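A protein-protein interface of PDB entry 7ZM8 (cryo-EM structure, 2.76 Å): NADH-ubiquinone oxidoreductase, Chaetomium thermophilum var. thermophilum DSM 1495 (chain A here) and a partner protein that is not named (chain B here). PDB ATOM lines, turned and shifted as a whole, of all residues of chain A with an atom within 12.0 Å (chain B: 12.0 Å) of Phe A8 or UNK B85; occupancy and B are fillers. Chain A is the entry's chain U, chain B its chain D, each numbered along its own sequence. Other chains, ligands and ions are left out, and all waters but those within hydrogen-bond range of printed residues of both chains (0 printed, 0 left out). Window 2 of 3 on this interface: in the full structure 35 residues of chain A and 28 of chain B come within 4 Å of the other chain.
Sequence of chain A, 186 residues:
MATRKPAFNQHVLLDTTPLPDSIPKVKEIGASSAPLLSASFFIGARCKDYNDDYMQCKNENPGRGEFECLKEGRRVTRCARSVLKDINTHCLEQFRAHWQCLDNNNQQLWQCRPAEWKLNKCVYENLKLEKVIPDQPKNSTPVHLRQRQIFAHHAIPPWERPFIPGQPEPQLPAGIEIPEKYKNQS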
ATOM      1  N   MET A   1      17.033  -8.560 -16.259  1.00  0.00           N
ATOM      2  CA  MET A   1      17.136  -9.407 -15.046  1.00  0.00           C
ATOM      3  C   MET A   1      18.507 -10.040 -15.015  1.00  0.00           C
ATOM      4  O   MET A   1      19.233  -9.848 -15.986  1.00  0.00           O
ATOM      5  CB  MET A   1      16.062 -10.486 -15.007  1.00  0.00           C
ATOM      6  N   ALA A   2      18.805 -10.832 -13.997  1.00  0.00           N
ATOM      7  CA  ALA A   2      20.182 -11.336 -13.827  1.00  0.00           C
ATOM      8  C   ALA A   2      20.664 -12.111 -15.041  1.00  0.00           C
ATOM      9  O   ALA A   2      19.875 -12.834 -15.629  1.00  0.00           O
ATOM     10  CB  ALA A   2      20.278 -12.136 -12.573  1.00  0.00           C
ATOM     11  N   THR A   3      21.943 -11.954 -15.388  1.00  0.00           N
ATOM     12  CA  THR A   3      22.520 -12.597 -16.595  1.00  0.00           C
ATOM     13  C   THR A   3      23.002 -14.011 -16.282  1.00  0.00           C
ATOM     14  O   THR A   3      23.533 -14.662 -17.188  1.00  0.00           O
ATOM     15  CB  THR A   3      23.685 -11.768 -17.138  1.00  0.00           C
ATOM     16  OG1 THR A   3      24.657 -11.645 -16.102  1.00  0.00           O
ATOM     17  CG2 THR A   3      23.273 -10.391 -17.601  1.00  0.00           C
ATOM     18  N   ARG A   4      22.841 -14.463 -15.050  1.00  0.00           N
ATOM     19  CA  ARG A   4      23.205 -15.848 -14.684  1.00  0.00           C
ATOM     20  C   ARG A   4      22.371 -16.823 -15.497  1.00  0.00           C
ATOM     21  O   ARG A   4      21.191 -16.562 -15.670  1.00  0.00           O
ATOM     22  CB  ARG A   4      22.859 -16.078 -13.213  1.00  0.00           C
ATOM     23  CG  ARG A   4      23.013 -17.517 -12.753  1.00  0.00           C
ATOM     24  CD  ARG A   4      22.549 -17.732 -11.331  1.00  0.00           C
ATOM     25  NE  ARG A   4      21.306 -17.055 -11.007  1.00  0.00           N
ATOM     26  CZ  ARG A   4      20.101 -17.599 -11.086  1.00  0.00           C
ATOM     27  NH1 ARG A   4      19.036 -16.892 -10.754  1.00  0.00           N
ATOM     28  NH2 ARG A   4      19.962 -18.847 -11.497  1.00  0.00           N
ATOM     29  N   LYS A   5      22.983 -17.893 -16.004  1.00  0.00           N
ATOM     30  CA  LYS A   5      22.215 -18.945 -16.697  1.00  0.00           C
ATOM     31  C   LYS A   5      21.337 -19.625 -15.641  1.00  0.00           C
ATOM     32  O   LYS A   5      21.856 -19.926 -14.554  1.00  0.00           O
ATOM     33  CB  LYS A   5      23.226 -19.915 -17.290  1.00  0.00           C
ATOM     34  CG  LYS A   5      24.176 -19.323 -18.321  1.00  0.00           C
ATOM     35  CD  LYS A   5      25.420 -20.160 -18.521  1.00  0.00           C
ATOM     36  CE  LYS A   5      25.981 -20.062 -19.922  1.00  0.00           C
ATOM     37  NZ  LYS A   5      25.115 -20.759 -20.901  1.00  0.00           N
ATOM     38  N   PRO A   6      20.040 -19.896 -15.894  1.00  0.00           N
ATOM     39  CA  PRO A   6      19.224 -20.580 -14.905  1.00  0.00           C
ATOM     40  C   PRO A   6      19.385 -22.112 -14.830  1.00  0.00           C
ATOM     41  O   PRO A   6      19.568 -22.726 -15.853  1.00  0.00           O
ATOM     42  CB  PRO A   6      17.835 -20.109 -15.330  1.00  0.00           C
ATOM     43  CG  PRO A   6      17.909 -20.001 -16.829  1.00  0.00           C
ATOM     44  CD  PRO A   6      19.315 -19.522 -17.106  1.00  0.00           C
ATOM     45  N   ALA A   7      19.275 -22.691 -13.628  1.00  0.00           N
ATOM     46  CA  ALA A   7      19.430 -24.127 -13.476  1.00  0.00           C
ATOM     47  C   ALA A   7      18.135 -24.862 -13.174  1.00  0.00           C
ATOM     48  O   ALA A   7      17.997 -26.016 -13.587  1.00  0.00           O
ATOM     49  CB  ALA A   7      20.442 -24.439 -12.360  1.00  0.00           C
ATOM     50  N   PHE A   8      17.209 -24.207 -12.478  1.00  0.00           N
ATOM     51  CA  PHE A   8      15.945 -24.859 -12.061  1.00  0.00           C
ATOM     52  C   PHE A   8      14.763 -23.966 -12.451  1.00  0.00           C
ATOM     53  O   PHE A   8      13.867 -23.770 -11.621  1.00  0.00           O
ATOM     54  CB  PHE A   8      15.978 -25.147 -10.559  1.00  0.00           C
ATOM     55  CG  PHE A   8      17.236 -25.817 -10.075  1.00  0.00           C
ATOM     56  CD1 PHE A   8      17.485 -27.148 -10.357  1.00  0.00           C
ATOM     57  CD2 PHE A   8      18.172 -25.114  -9.337  1.00  0.00           C
ATOM     58  CE1 PHE A   8      18.648 -27.757  -9.920  1.00  0.00           C
ATOM     59  CE2 PHE A   8      19.335 -25.723  -8.900  1.00  0.00           C
ATOM     60  CZ  PHE A   8      19.570 -27.043  -9.196  1.00  0.00           C
ATOM     61  N   ASN A   9      14.770 -23.428 -13.668  1.00  0.00           N
ATOM     62  CA  ASN A   9      13.685 -22.529 -14.140  1.00  0.00           C
ATOM     63  C   ASN A   9      12.490 -23.370 -14.592  1.00  0.00           C
ATOM     64  O   ASN A   9      12.678 -24.203 -15.465  1.00  0.00           O
ATOM     65  CB  ASN A   9      14.166 -21.639 -15.289  1.00  0.00           C
ATOM     66  CG  ASN A   9      15.008 -22.361 -16.323  1.00  0.00           C
ATOM     67  OD1 ASN A   9      15.928 -23.104 -15.989  1.00  0.00           O
ATOM     68  ND2 ASN A   9      14.723 -22.127 -17.591  1.00  0.00           N
ATOM     69  N   GLN A  10      11.305 -23.145 -14.021  1.00  0.00           N
ATOM     70  CA  GLN A  10      10.097 -23.873 -14.483  1.00  0.00           C
ATOM     71  C   GLN A  10       9.022 -22.891 -14.943  1.00  0.00           C
ATOM     72  O   GLN A  10       8.071 -23.342 -15.589  1.00  0.00           O
ATOM     73  CB  GLN A  10       9.553 -24.751 -13.351  1.00  0.00           C
ATOM     74  CG  GLN A  10      10.548 -25.781 -12.835  1.00  0.00           C
ATOM     75  CD  GLN A  10      10.773 -26.903 -13.816  1.00  0.00           C
ATOM     76  OE1 GLN A  10       9.937 -27.194 -14.666  1.00  0.00           O
ATOM     77  NE2 GLN A  10      11.915 -27.556 -13.695  1.00  0.00           N
ATOM     78  N   HIS A  11       9.180 -21.603 -14.637  1.00  0.00           N
ATOM     79  CA  HIS A  11       8.116 -20.609 -14.943  1.00  0.00           C
ATOM     80  C   HIS A  11       8.690 -19.366 -15.623  1.00  0.00           C
ATOM     81  O   HIS A  11       9.860 -19.052 -15.385  1.00  0.00           O
ATOM     82  CB  HIS A  11       7.345 -20.246 -13.663  1.00  0.00           C
ATOM     83  CG  HIS A  11       6.629 -21.394 -13.038  1.00  0.00           C
ATOM     84  ND1 HIS A  11       5.511 -21.962 -13.610  1.00  0.00           N
ATOM     85  CD2 HIS A  11       6.861 -22.076 -11.898  1.00  0.00           C
ATOM     86  CE1 HIS A  11       5.086 -22.950 -12.852  1.00  0.00           C
ATOM     87  NE2 HIS A  11       5.897 -23.039 -11.795  1.00  0.00           N
ATOM     88  N   VAL A  12       7.874 -18.683 -16.428  1.00  0.00           N
ATOM     89  CA  VAL A  12       8.302 -17.446 -17.140  1.00  0.00           C
ATOM     90  C   VAL A  12       7.442 -16.291 -16.627  1.00  0.00           C
ATOM     91  O   VAL A  12       6.229 -16.494 -16.477  1.00  0.00           O
ATOM     92  CB  VAL A  12       8.177 -17.610 -18.666  1.00  0.00           C
ATOM     93  CG1 VAL A  12       8.009 -16.280 -19.380  1.00  0.00           C
ATOM     94  CG2 VAL A  12       9.342 -18.391 -19.250  1.00  0.00           C
ATOM     95  N   LEU A  13       8.060 -15.152 -16.316  1.00  0.00           N
ATOM     96  CA  LEU A  13       7.275 -13.961 -15.905  1.00  0.00           C
ATOM     97  C   LEU A  13       7.231 -12.962 -17.058  1.00  0.00           C
ATOM     98  O   LEU A  13       8.297 -12.476 -17.450  1.00  0.00           O
ATOM     99  CB  LEU A  13       7.879 -13.335 -14.646  1.00  0.00           C
ATOM    100  CG  LEU A  13       7.104 -12.160 -14.054  1.00  0.00           C
ATOM    101  CD1 LEU A  13       5.693 -12.572 -13.676  1.00  0.00           C
ATOM    102  CD2 LEU A  13       7.833 -11.593 -12.849  1.00  0.00           C
ATOM    103  N   GLU B  51      15.417 -19.176 -28.508  1.00  0.00           N
ATOM    104  CA  GLU B  51      14.333 -18.642 -27.650  1.00  0.00           C
ATOM    105  C   GLU B  51      13.637 -17.497 -28.375  1.00  0.00           C
ATOM    106  O   GLU B  51      12.434 -17.337 -28.187  1.00  0.00           O
ATOM    107  CB  GLU B  51      14.874 -18.367 -26.252  1.00  0.00           C
ATOM    108  CG  GLU B  51      15.055 -19.627 -25.435  1.00  0.00           C
ATOM    109  CD  GLU B  51      15.267 -19.392 -23.954  1.00  0.00           C
ATOM    110  OE1 GLU B  51      15.010 -18.264 -23.499  1.00  0.00           O
ATOM    111  OE2 GLU B  51      15.687 -20.339 -23.261  1.00  0.00           O
ATOM    112  N   TRP B  79      11.279 -13.940 -19.183  1.00  0.00           N
ATOM    113  CA  TRP B  79      12.268 -13.837 -18.083  1.00  0.00           C
ATOM    114  C   TRP B  79      12.100 -15.055 -17.184  1.00  0.00           C
ATOM    115  O   TRP B  79      11.090 -15.123 -16.477  1.00  0.00           O
ATOM    116  CB  TRP B  79      12.110 -12.515 -17.323  1.00  0.00           C
ATOM    117  CG  TRP B  79      12.650 -11.304 -18.021  1.00  0.00           C
ATOM    118  CD1 TRP B  79      12.953 -11.179 -19.344  1.00  0.00           C
ATOM    119  CD2 TRP B  79      12.945 -10.028 -17.422  1.00  0.00           C
ATOM    120  NE1 TRP B  79      13.417  -9.921 -19.611  1.00  0.00           N
ATOM    121  CE2 TRP B  79      13.424  -9.192 -18.451  1.00  0.00           C
ATOM    122  CE3 TRP B  79      12.847  -9.509 -16.127  1.00  0.00           C
ATOM    123  CZ2 TRP B  79      13.810  -7.873 -18.221  1.00  0.00           C
ATOM    124  CZ3 TRP B  79      13.226  -8.207 -15.900  1.00  0.00           C
ATOM    125  CH2 TRP B  79      13.704  -7.402 -16.934  1.00  0.00           C
ATOM    126  N   LYS B  80      13.042 -15.988 -17.240  1.00  0.00           N
ATOM    127  CA  LYS B  80      12.936 -17.242 -16.460  1.00  0.00           C
ATOM    128  C   LYS B  80      12.903 -16.926 -14.966  1.00  0.00           C
ATOM    129  O   LYS B  80      13.668 -16.065 -14.523  1.00  0.00           O
ATOM    130  CB  LYS B  80      14.118 -18.155 -16.791  1.00  0.00           C
ATOM    131  CG  LYS B  80      14.380 -18.399 -18.270  1.00  0.00           C
ATOM    132  CD  LYS B  80      13.141 -18.736 -19.064  1.00  0.00           C
ATOM    133  CE  LYS B  80      13.438 -19.218 -20.466  1.00  0.00           C
ATOM    134  NZ  LYS B  80      14.156 -20.514 -20.457  1.00  0.00           N
ATOM    135  N   VAL B  81      11.962 -17.656 -14.250  1.00  0.00           N
ATOM    136  CA  VAL B  81      11.846 -17.493 -12.772  1.00  0.00           C
ATOM    137  C   VAL B  81      12.265 -18.804 -12.097  1.00  0.00           C
ATOM    138  O   VAL B  81      11.841 -19.868 -12.580  1.00  0.00           O
ATOM    139  CB  VAL B  81      10.449 -17.008 -12.334  1.00  0.00           C
ATOM    140  CG1 VAL B  81      10.556 -15.954 -11.249  1.00  0.00           C
ATOM    141  CG2 VAL B  81       9.635 -16.468 -13.494  1.00  0.00           C
ATOM    142  N   UNK B  82      13.133 -18.695 -11.024  1.00  0.00           N
ATOM    143  CA  UNK B  82      13.602 -19.910 -10.320  1.00  0.00           C
ATOM    144  C   UNK B  82      13.250 -19.757  -8.847  1.00  0.00           C
ATOM    145  O   UNK B  82      12.892 -18.650  -8.445  1.00  0.00           O
ATOM    146  CB  UNK B  82      15.086 -20.112 -10.510  1.00  0.00           C
ATOM    147  N   UNK B  83      13.387 -20.831  -8.080  1.00  0.00           N
ATOM    148  CA  UNK B  83      13.130 -20.766  -6.629  1.00  0.00           C
ATOM    149  C   UNK B  83      14.415 -20.924  -5.817  1.00  0.00           C
ATOM    150  O   UNK B  83      14.460 -20.358  -4.712  1.00  0.00           O
ATOM    151  CB  UNK B  83      12.138 -21.835  -6.263  1.00  0.00           C
ATOM    152  N   UNK B  84      15.425 -21.648  -6.322  1.00  0.00           N
ATOM    153  CA  UNK B  84      16.574 -21.911  -5.466  1.00  0.00           C
ATOM    154  C   UNK B  84      17.894 -21.440  -6.055  1.00  0.00           C
ATOM    155  O   UNK B  84      18.644 -20.731  -5.375  1.00  0.00           O
ATOM    156  CB  UNK B  84      16.652 -23.411  -5.132  1.00  0.00           C
ATOM    157  N   UNK B  85      18.180 -21.807  -7.307  1.00  0.00           N
ATOM    158  CA  UNK B  85      19.502 -21.449  -7.882  1.00  0.00           C
ATOM    159  C   UNK B  85      19.756 -19.945  -7.893  1.00  0.00           C
ATOM    160  O   UNK B  85      18.795 -19.173  -8.019  1.00  0.00           O
ATOM    161  CB  UNK B  85      19.671 -22.010  -9.256  1.00  0.00           C
ATOM    162  N   UNK B  86      21.022 -19.562  -7.826  1.00  0.00           N
ATOM    163  CA  UNK B  86      21.338 -18.130  -7.700  1.00  0.00           C
ATOM    164  C   UNK B  86      22.812 -17.930  -8.039  1.00  0.00           C
ATOM    165  O   UNK B  86      23.288 -16.828  -7.731  1.00  0.00           O
ATOM    166  CB  UNK B  86      21.028 -17.668  -6.305  1.00  0.00           C
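The side-chain amino group (NZ) of Lys B80 lies close to the side-chain amide nitrogen (ND2) of Asn A9. The backbone carbonyl oxygen (O) of His A11 lies within hydrogen-bond range of the backbone NH (N) of Val B81 (2.8 Å). The backbone NH of Leu A13 sits at hydrogen-bond distance from the backbone carbonyl oxygen of Trp B79 (3.0 Å).
The side-chain amino group of Lys B80 lies within salt-bridge range of the side-chain carboxylate of Glu B51 (3.2 Å).
Among the printed residues, pairs that only touch across the chains: Met A1 with Trp B79 (3.5 Å), Arg A4 with UNK B85 (3.6 Å), Arg A4 with UNK B86 (3.3 Å), Phe A8 with UNK B85 (3.4 Å), Asn A9 with Val B81 (3.6 Å), Gln A10 with Val B81 (3.6 Å), His A11 with Lys B80 (3.7 Å), Val A12 with Trp B79 (3.7 Å), Val A12 with Lys B80 (3.8 Å), Val A12 with Val B81 (3.8 Å) and Leu A13 with Val B81 (3.5 Å).
No residue of chain B comes within 4 Å of Pro A6. Of the printed residues of chain B, Phe A8 touches UNK B85. Of chain B, only Lys B80 (3.3 Å) and Val B81 (3.6 Å) come within 4 Å of Asn A9. Of the printed residues of chain B, Gln A10 touches Val B81. Of the printed residues of chain B, Val A12 touches Trp B79, Lys B80 and Val B81. Of the printed residues of chain A, Trp B79 touches Met A1, Val A12 and Leu A13. Of the printed residues of chain A, Lys B80 touches Asn A9, His A11 and Val A12. Of the printed residues of chain A, Val B81 touches Asn A9, Gln A10, His A11, Val A12 and Leu A13. No residue of chain A comes within 4 Å of UNK B83. No residue of chain A comes within 4 Å of UNK B84. Printed residues of chain A within 4 Å of UNK B85: Arg A4 and Phe A8. UNK B86 touches just one residue of chain A: Arg A4 (3.3 Å).
Of the 13 printed residues of chain A, 8 touch a printed residue of chain B. Printed residues of chain A that touch a printed residue of chain B: Met A1, Arg A4, Phe A8, Asn A9, Gln A10, His A11, Val A12 and Leu A13. Hydrophobic or aromatic side chains of chain A that line the printed part of chain B: Met A1, Phe A8, Val A12 and Leu A13. Among the printed residues, 14 pairs touch across the chains.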
